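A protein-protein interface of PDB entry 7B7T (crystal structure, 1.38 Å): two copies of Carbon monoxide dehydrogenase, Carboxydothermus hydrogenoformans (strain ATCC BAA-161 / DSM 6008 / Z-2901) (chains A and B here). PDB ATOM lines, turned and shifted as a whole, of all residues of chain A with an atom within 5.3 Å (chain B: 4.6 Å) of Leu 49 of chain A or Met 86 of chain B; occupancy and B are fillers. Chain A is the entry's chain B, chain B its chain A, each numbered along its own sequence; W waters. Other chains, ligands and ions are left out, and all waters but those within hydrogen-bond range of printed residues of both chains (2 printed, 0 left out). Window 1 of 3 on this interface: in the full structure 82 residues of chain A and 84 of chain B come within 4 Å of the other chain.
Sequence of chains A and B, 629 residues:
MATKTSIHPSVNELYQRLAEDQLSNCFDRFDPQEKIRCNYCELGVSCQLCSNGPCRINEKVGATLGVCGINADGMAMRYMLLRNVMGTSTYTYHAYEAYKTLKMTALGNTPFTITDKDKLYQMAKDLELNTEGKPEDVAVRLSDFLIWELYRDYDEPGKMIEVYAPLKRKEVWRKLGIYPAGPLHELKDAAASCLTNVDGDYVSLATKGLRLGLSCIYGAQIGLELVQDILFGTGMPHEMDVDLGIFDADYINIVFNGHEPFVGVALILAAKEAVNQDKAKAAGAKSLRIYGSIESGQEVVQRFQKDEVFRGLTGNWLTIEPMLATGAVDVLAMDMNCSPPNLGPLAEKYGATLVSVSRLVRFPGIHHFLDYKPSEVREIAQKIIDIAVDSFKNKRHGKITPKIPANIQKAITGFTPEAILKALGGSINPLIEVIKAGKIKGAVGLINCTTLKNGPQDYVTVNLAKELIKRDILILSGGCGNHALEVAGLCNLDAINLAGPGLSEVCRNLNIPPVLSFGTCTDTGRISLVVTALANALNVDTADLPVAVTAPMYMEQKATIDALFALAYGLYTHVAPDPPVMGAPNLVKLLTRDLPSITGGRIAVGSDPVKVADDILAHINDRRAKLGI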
ATOM      1  N   CYS A  47       5.529  28.109   7.711  1.00  0.00           N
ATOM      2  CA  CYS A  47       5.677  26.698   8.031  1.00  0.00           C
ATOM      3  C   CYS A  47       5.544  26.524   9.531  1.00  0.00           C
ATOM      4  O   CYS A  47       6.119  27.292  10.311  1.00  0.00           O
ATOM      5  CB  CYS A  47       7.041  26.190   7.545  1.00  0.00           C
ATOM      6  SG  CYS A  47       7.258  24.403   7.768  1.00  0.00           S
ATOM      7  N   GLN A  48       4.846  25.453   9.925  1.00  0.00           N
ATOM      8  CA  GLN A  48       4.639  25.089  11.328  1.00  0.00           C
ATOM      9  C   GLN A  48       5.033  23.645  11.617  1.00  0.00           C
ATOM     10  O   GLN A  48       4.512  23.047  12.564  1.00  0.00           O
ATOM     11  CB  GLN A  48       3.186  25.314  11.751  1.00  0.00           C
ATOM     12  CG  GLN A  48       2.654  26.711  11.457  1.00  0.00           C
ATOM     13  CD  GLN A  48       2.283  26.934   9.993  1.00  0.00           C
ATOM     14  OE1 GLN A  48       1.886  26.002   9.274  1.00  0.00           O
ATOM     15  NE2 GLN A  48       2.413  28.181   9.541  1.00  0.00           N
ATOM     16  N   LEU A  49       5.924  23.058  10.836  1.00  0.00           N
ATOM     17  CA  LEU A  49       6.089  21.607  10.928  1.00  0.00           C
ATOM     18  C   LEU A  49       7.062  21.136  11.983  1.00  0.00           C
ATOM     19  O   LEU A  49       7.108  19.935  12.202  1.00  0.00           O
ATOM     20  CB  LEU A  49       6.519  21.027   9.579  1.00  0.00           C
ATOM     21  CG  LEU A  49       5.515  21.172   8.445  1.00  0.00           C
ATOM     22  CD1 LEU A  49       6.026  20.496   7.200  1.00  0.00           C
ATOM     23  CD2 LEU A  49       4.146  20.646   8.854  1.00  0.00           C
ATOM     24  N   CYS A  50       7.835  22.010  12.624  1.00  0.00           N
ATOM     25  CA  CYS A  50       8.739  21.552  13.662  1.00  0.00           C
ATOM     26  C   CYS A  50       8.951  22.621  14.733  1.00  0.00           C
ATOM     27  O   CYS A  50       8.560  23.788  14.588  1.00  0.00           O
ATOM     28  CB  CYS A  50      10.066  21.072  13.078  1.00  0.00           C
ATOM     29  SG  CYS A  50      11.309  22.350  12.869  1.00  0.00           S
ATOM     30  N   SER A  51       9.624  22.215  15.817  1.00  0.00           N
ATOM     31  CA  SER A  51       9.741  23.103  16.971  1.00  0.00           C
ATOM     32  C   SER A  51      10.693  24.273  16.754  1.00  0.00           C
ATOM     33  O   SER A  51      10.652  25.219  17.547  1.00  0.00           O
ATOM     34  CB  SER A  51      10.169  22.355  18.218  1.00  0.00           C
ATOM     35  OG  SER A  51      11.548  22.016  18.187  1.00  0.00           O
ATOM     36  N   ARG A  78       5.777  21.430  -0.090  1.00  0.00           N
ATOM     37  CA  ARG A  78       5.686  20.412   0.958  1.00  0.00           C
ATOM     38  C   ARG A  78       4.342  20.456   1.674  1.00  0.00           C
ATOM     39  O   ARG A  78       3.729  19.409   1.935  1.00  0.00           O
ATOM     40  CB  ARG A  78       6.846  20.566   1.946  1.00  0.00           C
ATOM     41  CG  ARG A  78       6.830  19.538   3.052  1.00  0.00           C
ATOM     42  CD  ARG A  78       8.124  19.620   3.870  1.00  0.00           C
ATOM     43  NE  ARG A  78       8.248  20.937   4.490  1.00  0.00           N
ATOM     44  CZ  ARG A  78       9.237  21.287   5.294  1.00  0.00           C
ATOM     45  NH1 ARG A  78      10.192  20.407   5.553  1.00  0.00           N
ATOM     46  NH2 ARG A  78       9.284  22.504   5.821  1.00  0.00           N
ATOM     47  N   LEU A  82       1.505  17.571   1.832  1.00  0.00           N
ATOM     48  CA  LEU A  82       0.951  17.066   3.083  1.00  0.00           C
ATOM     49  C   LEU A  82      -0.560  17.154   3.069  1.00  0.00           C
ATOM     50  O   LEU A  82      -1.267  16.205   3.450  1.00  0.00           O
ATOM     51  CB  LEU A  82       1.525  17.827   4.277  1.00  0.00           C
ATOM     52  CG  LEU A  82       1.016  17.471   5.673  1.00  0.00           C
ATOM     53  CD1 LEU A  82       1.360  16.028   5.996  1.00  0.00           C
ATOM     54  CD2 LEU A  82       1.598  18.389   6.745  1.00  0.00           C
ATOM     55  N   ALA A 191       3.713  11.374   3.011  1.00  0.00           N
ATOM     56  CA  ALA A 191       3.725  11.932   4.363  1.00  0.00           C
ATOM     57  C   ALA A 191       5.118  11.878   4.978  1.00  0.00           C
ATOM     58  O   ALA A 191       5.581  12.837   5.594  1.00  0.00           O
ATOM     59  CB  ALA A 191       2.711  11.235   5.258  1.00  0.00           C
ATOM     60  N   ALA A 192       5.819  10.762   4.798  1.00  0.00           N
ATOM     61  CA  ALA A 192       7.173  10.643   5.329  1.00  0.00           C
ATOM     62  C   ALA A 192       8.111  11.645   4.685  1.00  0.00           C
ATOM     63  O   ALA A 192       9.021  12.164   5.341  1.00  0.00           O
ATOM     64  CB  ALA A 192       7.682   9.226   5.125  1.00  0.00           C
ATOM     65  N   CYS A 194       7.420  14.607   3.866  1.00  0.00           N
ATOM     66  CA  CYS A 194       7.112  15.939   4.382  1.00  0.00           C
ATOM     67  C   CYS A 194       7.633  16.184   5.788  1.00  0.00           C
ATOM     68  O   CYS A 194       7.641  17.334   6.235  1.00  0.00           O
ATOM     69  CB  CYS A 194       5.608  16.172   4.395  1.00  0.00           C
ATOM     70  SG  CYS A 194       4.862  16.256   2.721  1.00  0.00           S
ATOM     71  N   LEU A 195       8.102  15.156   6.492  1.00  0.00           N
ATOM     72  CA  LEU A 195       8.715  15.413   7.780  1.00  0.00           C
ATOM     73  C   LEU A 195       9.928  16.320   7.598  1.00  0.00           C
ATOM     74  O   LEU A 195      10.611  16.283   6.579  1.00  0.00           O
ATOM     75  CB  LEU A 195       9.132  14.097   8.451  1.00  0.00           C
ATOM     76  CG  LEU A 195       9.452  14.155   9.938  1.00  0.00           C
ATOM     77  CD1 LEU A 195       8.297  13.659  10.765  1.00  0.00           C
ATOM     78  CD2 LEU A 195      10.728  13.381  10.230  1.00  0.00           C
ATOM     79  N   THR A 196      10.193  17.134   8.613  1.00  0.00           N
ATOM     80  CA  THR A 196      11.322  18.055   8.581  1.00  0.00           C
ATOM     81  C   THR A 196      12.609  17.317   8.221  1.00  0.00           C
ATOM     82  O   THR A 196      12.876  16.202   8.682  1.00  0.00           O
ATOM     83  CB  THR A 196      11.453  18.747   9.940  1.00  0.00           C
ATOM     84  OG1 THR A 196      10.194  19.365  10.260  1.00  0.00           O
ATOM     85  CG2 THR A 196      12.584  19.763   9.916  1.00  0.00           C
ATOM     86  N   TYR B  79      -4.127  19.782  13.886  1.00  0.00           N
ATOM     87  CA  TYR B  79      -2.832  19.931  13.250  1.00  0.00           C
ATOM     88  C   TYR B  79      -1.805  19.047  13.950  1.00  0.00           C
ATOM     89  O   TYR B  79      -0.914  18.487  13.309  1.00  0.00           O
ATOM     90  CB  TYR B  79      -2.430  21.407  13.241  1.00  0.00           C
ATOM     91  CG  TYR B  79      -1.443  21.905  12.185  1.00  0.00           C
ATOM     92  CD1 TYR B  79      -0.840  21.076  11.274  1.00  0.00           C
ATOM     93  CD2 TYR B  79      -1.077  23.239  12.164  1.00  0.00           C
ATOM     94  CE1 TYR B  79       0.086  21.551  10.369  1.00  0.00           C
ATOM     95  CE2 TYR B  79      -0.155  23.738  11.252  1.00  0.00           C
ATOM     96  CZ  TYR B  79       0.416  22.890  10.363  1.00  0.00           C
ATOM     97  OH  TYR B  79       1.331  23.340   9.452  1.00  0.00           O
ATOM     98  N   LEU B  82      -2.294  15.654  12.396  1.00  0.00           N
ATOM     99  CA  LEU B  82      -1.773  15.584  11.042  1.00  0.00           C
ATOM    100  C   LEU B  82      -0.261  15.483  11.068  1.00  0.00           C
ATOM    101  O   LEU B  82       0.335  14.677  10.342  1.00  0.00           O
ATOM    102  CB  LEU B  82      -2.231  16.827  10.264  1.00  0.00           C
ATOM    103  CG  LEU B  82      -1.730  16.934   8.828  1.00  0.00           C
ATOM    104  CD1 LEU B  82      -2.244  15.771   7.967  1.00  0.00           C
ATOM    105  CD2 LEU B  82      -2.170  18.277   8.205  1.00  0.00           C
ATOM    106  N   ARG B  83       0.393  16.344  11.846  1.00  0.00           N
ATOM    107  CA  ARG B  83       1.844  16.300  11.872  1.00  0.00           C
ATOM    108  C   ARG B  83       2.312  14.926  12.342  1.00  0.00           C
ATOM    109  O   ARG B  83       3.292  14.386  11.819  1.00  0.00           O
ATOM    110  CB  ARG B  83       2.432  17.484  12.657  1.00  0.00           C
ATOM    111  CG  ARG B  83       2.382  18.818  11.894  1.00  0.00           C
ATOM    112  CD  ARG B  83       3.036  19.927  12.701  1.00  0.00           C
ATOM    113  NE  ARG B  83       2.283  20.134  13.920  1.00  0.00           N
ATOM    114  CZ  ARG B  83       1.680  21.259  14.276  1.00  0.00           C
ATOM    115  NH1 ARG B  83       1.817  22.359  13.560  1.00  0.00           N
ATOM    116  NH2 ARG B  83       0.970  21.296  15.394  1.00  0.00           N
ATOM    117  N   ASN B  84       1.569  14.307  13.281  1.00  0.00           N
ATOM    118  CA  ASN B  84       1.919  12.979  13.777  1.00  0.00           C
ATOM    119  C   ASN B  84       1.620  11.828  12.814  1.00  0.00           C
ATOM    120  O   ASN B  84       2.198  10.722  12.962  1.00  0.00           O
ATOM    121  CB  ASN B  84       1.271  12.764  15.106  1.00  0.00           C
ATOM    122  CG  ASN B  84       2.066  13.421  16.210  1.00  0.00           C
ATOM    123  OD1 ASN B  84       3.024  12.835  16.716  1.00  0.00           O
ATOM    124  ND2 ASN B  84       1.779  14.708  16.496  1.00  0.00           N
ATOM    125  N   VAL B  85       0.745  12.050  11.837  1.00  0.00           N
ATOM    126  CA  VAL B  85       0.686  11.147  10.688  1.00  0.00           C
ATOM    127  C   VAL B  85       2.051  11.059  10.019  1.00  0.00           C
ATOM    128  O   VAL B  85       2.488   9.980   9.605  1.00  0.00           O
ATOM    129  CB  VAL B  85      -0.403  11.605   9.706  1.00  0.00           C
ATOM    130  CG1 VAL B  85      -0.285  10.889   8.371  1.00  0.00           C
ATOM    131  CG2 VAL B  85      -1.766  11.374  10.323  1.00  0.00           C
ATOM    132  N   MET B  86       2.750  12.189   9.893  1.00  0.00           N
ATOM    133  CA  MET B  86       4.089  12.166   9.314  1.00  0.00           C
ATOM    134  C   MET B  86       5.017  11.290  10.153  1.00  0.00           C
ATOM    135  O   MET B  86       5.770  10.464   9.624  1.00  0.00           O
ATOM    136  CB  MET B  86       4.665  13.593   9.212  1.00  0.00           C
ATOM    137  CG  MET B  86       3.913  14.607   8.330  1.00  0.00           C
ATOM    138  SD  MET B  86       4.899  16.124   7.930  1.00  0.00           S
ATOM    139  CE  MET B  86       4.783  17.025   9.485  1.00  0.00           C
ATOM    140  N   GLY B  87       4.991  11.474  11.477  1.00  0.00           N
ATOM    141  CA  GLY B  87       5.855  10.671  12.330  1.00  0.00           C
ATOM    142  C   GLY B  87       5.576   9.190  12.183  1.00  0.00           C
ATOM    143  O   GLY B  87       6.502   8.377  12.010  1.00  0.00           O
ATOM    144  N   THR B  88       4.292   8.821  12.273  1.00  0.00           N
ATOM    145  CA  THR B  88       3.898   7.425  12.109  1.00  0.00           C
ATOM    146  C   THR B  88       4.323   6.896  10.739  1.00  0.00           C
ATOM    147  O   THR B  88       4.788   5.756  10.621  1.00  0.00           O
ATOM    148  CB  THR B  88       2.386   7.270  12.334  1.00  0.00           C
ATOM    149  OG1 THR B  88       2.010   7.814  13.609  1.00  0.00           O
ATOM    150  CG2 THR B  88       1.981   5.804  12.277  1.00  0.00           C
ATOM    151  N   SER B  89       4.170   7.712   9.692  1.00  0.00           N
ATOM    152  CA  SER B  89       4.528   7.257   8.358  1.00  0.00           C
ATOM    153  C   SER B  89       6.010   6.922   8.257  1.00  0.00           C
ATOM    154  O   SER B  89       6.387   5.977   7.560  1.00  0.00           O
ATOM    155  CB  SER B  89       4.150   8.317   7.322  1.00  0.00           C
ATOM    156  OG  SER B  89       2.729   8.466   7.234  1.00  0.00           O
ATOM    157  N   THR B  90       6.862   7.695   8.929  1.00  0.00           N
ATOM    158  CA  THR B  90       8.300   7.400   8.863  1.00  0.00           C
ATOM    159  C   THR B  90       8.625   6.070   9.532  1.00  0.00           C
ATOM    160  O   THR B  90       9.396   5.272   8.994  1.00  0.00           O
ATOM    161  CB  THR B  90       9.183   8.533   9.397  1.00  0.00           C
ATOM    162  OG1 THR B  90       9.048   8.697  10.805  1.00  0.00           O
ATOM    163  CG2 THR B  90       8.908   9.811   8.729  1.00  0.00           C
ATOM    164  N   GLN B 557       8.085  15.042  14.492  1.00  0.00           N
ATOM    165  CA  GLN B 557       6.986  14.250  15.043  1.00  0.00           C
ATOM    166  C   GLN B 557       7.288  12.784  15.224  1.00  0.00           C
ATOM    167  O   GLN B 557       6.435  12.040  15.722  1.00  0.00           O
ATOM    168  CB  GLN B 557       5.678  14.436  14.273  1.00  0.00           C
ATOM    169  CG  GLN B 557       5.179  15.795  14.402  1.00  0.00           C
ATOM    170  CD  GLN B 557       5.968  16.742  13.518  1.00  0.00           C
ATOM    171  OE1 GLN B 557       6.499  16.339  12.470  1.00  0.00           O
ATOM    172  NE2 GLN B 557       6.047  17.998  13.927  1.00  0.00           N
HETATM  173  O   HOH W   1       8.310  17.552  10.871  1.00  0.00           O
HETATM  174  O   HOH W   2       3.489  24.027   7.611  1.00  0.00           O
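Position printed for both chains: 82.
Of the printed residues of chain B, Leu 49 of chain A touches Tyr 79, Arg 83, Met 86 and Gln 557. Printed residues of chain B within 4 Å of Leu 195 of chain A: Met 86 and Gln 557. Printed residues of chain B within 4 Å of Ala 192 of chain A: Ser 89 and Thr 90. Of the printed residues of chain B, Leu 82 of chain A touches Met 86. Of the printed residues of chain B, Ala 191 of chain A touches Met 86 (3.7 Å) and Ser 89 (3.4 Å). Of the printed residues of chain A, Arg 83 of chain B touches Gln 48 and Leu 49. Arg 78 of chain A touches none of the printed residues of chain B. The nearest printed residue of chain B that does not touch Leu 195 of chain A is Gly 87 of chain B (4.03 Å).
Among the printed residues, pairs that only touch across the chains: Leu 49 of chain A with Tyr 79 of chain B (3.9 Å), Leu 49 of chain A with Arg 83 of chain B (3.9 Å), Leu 49 of chain A with Met 86 of chain B (3.7 Å), Leu 82 of chain A with Met 86 of chain B (3.7 Å), Ala 191 of chain A with Met 86 of chain B (3.7 Å), Ala 191 of chain A with Ser 89 of chain B (3.4 Å), Ala 192 of chain A with Ser 89 of chain B (3.9 Å), Ala 192 of chain A with Thr 90 of chain B (3.9 Å) and Leu 195 of chain A with Gln 557 of chain B (3.6 Å).
The side-chain hydroxyl of Ser 89 of chain B lies within hydrogen-bond range of the backbone carbonyl oxygen of Val 85 of chain B, 2.8 Å away. O of Gly 87 of chain B lies within hydrogen-bond range of OG1 of Thr 90 of chain B. The side-chain sulfur (SG) of Cys 47 of chain A sits close to the backbone NH (N) of Leu 49 of chain A. The side-chain sulfur (SG) of Cys 194 of chain A lies within hydrogen-bond range of the backbone carbonyl oxygen (O) of Arg 78 of chain A (3.4 Å). N of Leu 82 of chain A is in hydrogen-bond range of SG of Cys 194 of chain A (3.7 Å).
Water W1 lies within hydrogen-bond range of the side-chain hydroxyl of Thr 196 of chain A (2.7 Å), the side-chain amide oxygen of Gln 557 of chain B (2.7 Å) and the backbone carbonyl oxygen of Leu 49 of chain A (3.0 Å). Water W2 lies within hydrogen-bond range of OH of Tyr 79 of chain B and N of Gln 48 of chain A.
Of the 11 printed residues of chain B, 6 touch a printed residue of chain A. Among the printed residues, no Asp or Glu carboxylate lies within 4 Å of a Lys or Arg side-chain nitrogen of the other chain.
OH of Tyr 79 of chain B lies within hydrogen-bond range of OE1 of Gln 48 of chain A (2.7 Å). NH1 of Arg 83 of chain B sits at hydrogen-bond distance from O of Gln 48 of chain A, 3.0 Å away. The side-chain sulfur (SD) of Met 86 of chain B is in hydrogen-bond range of the backbone NH (N) of Leu 195 of chain A (3.6 Å). The backbone carbonyl oxygen (O) of Leu 49 of chain A is in hydrogen-bond range of the side-chain amide nitrogen (NE2) of Gln 557 of chain B, at 2.8 Å. O of Cys 194 of chain A sits close to SD of Met 86 of chain B, at 3.4 Å.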
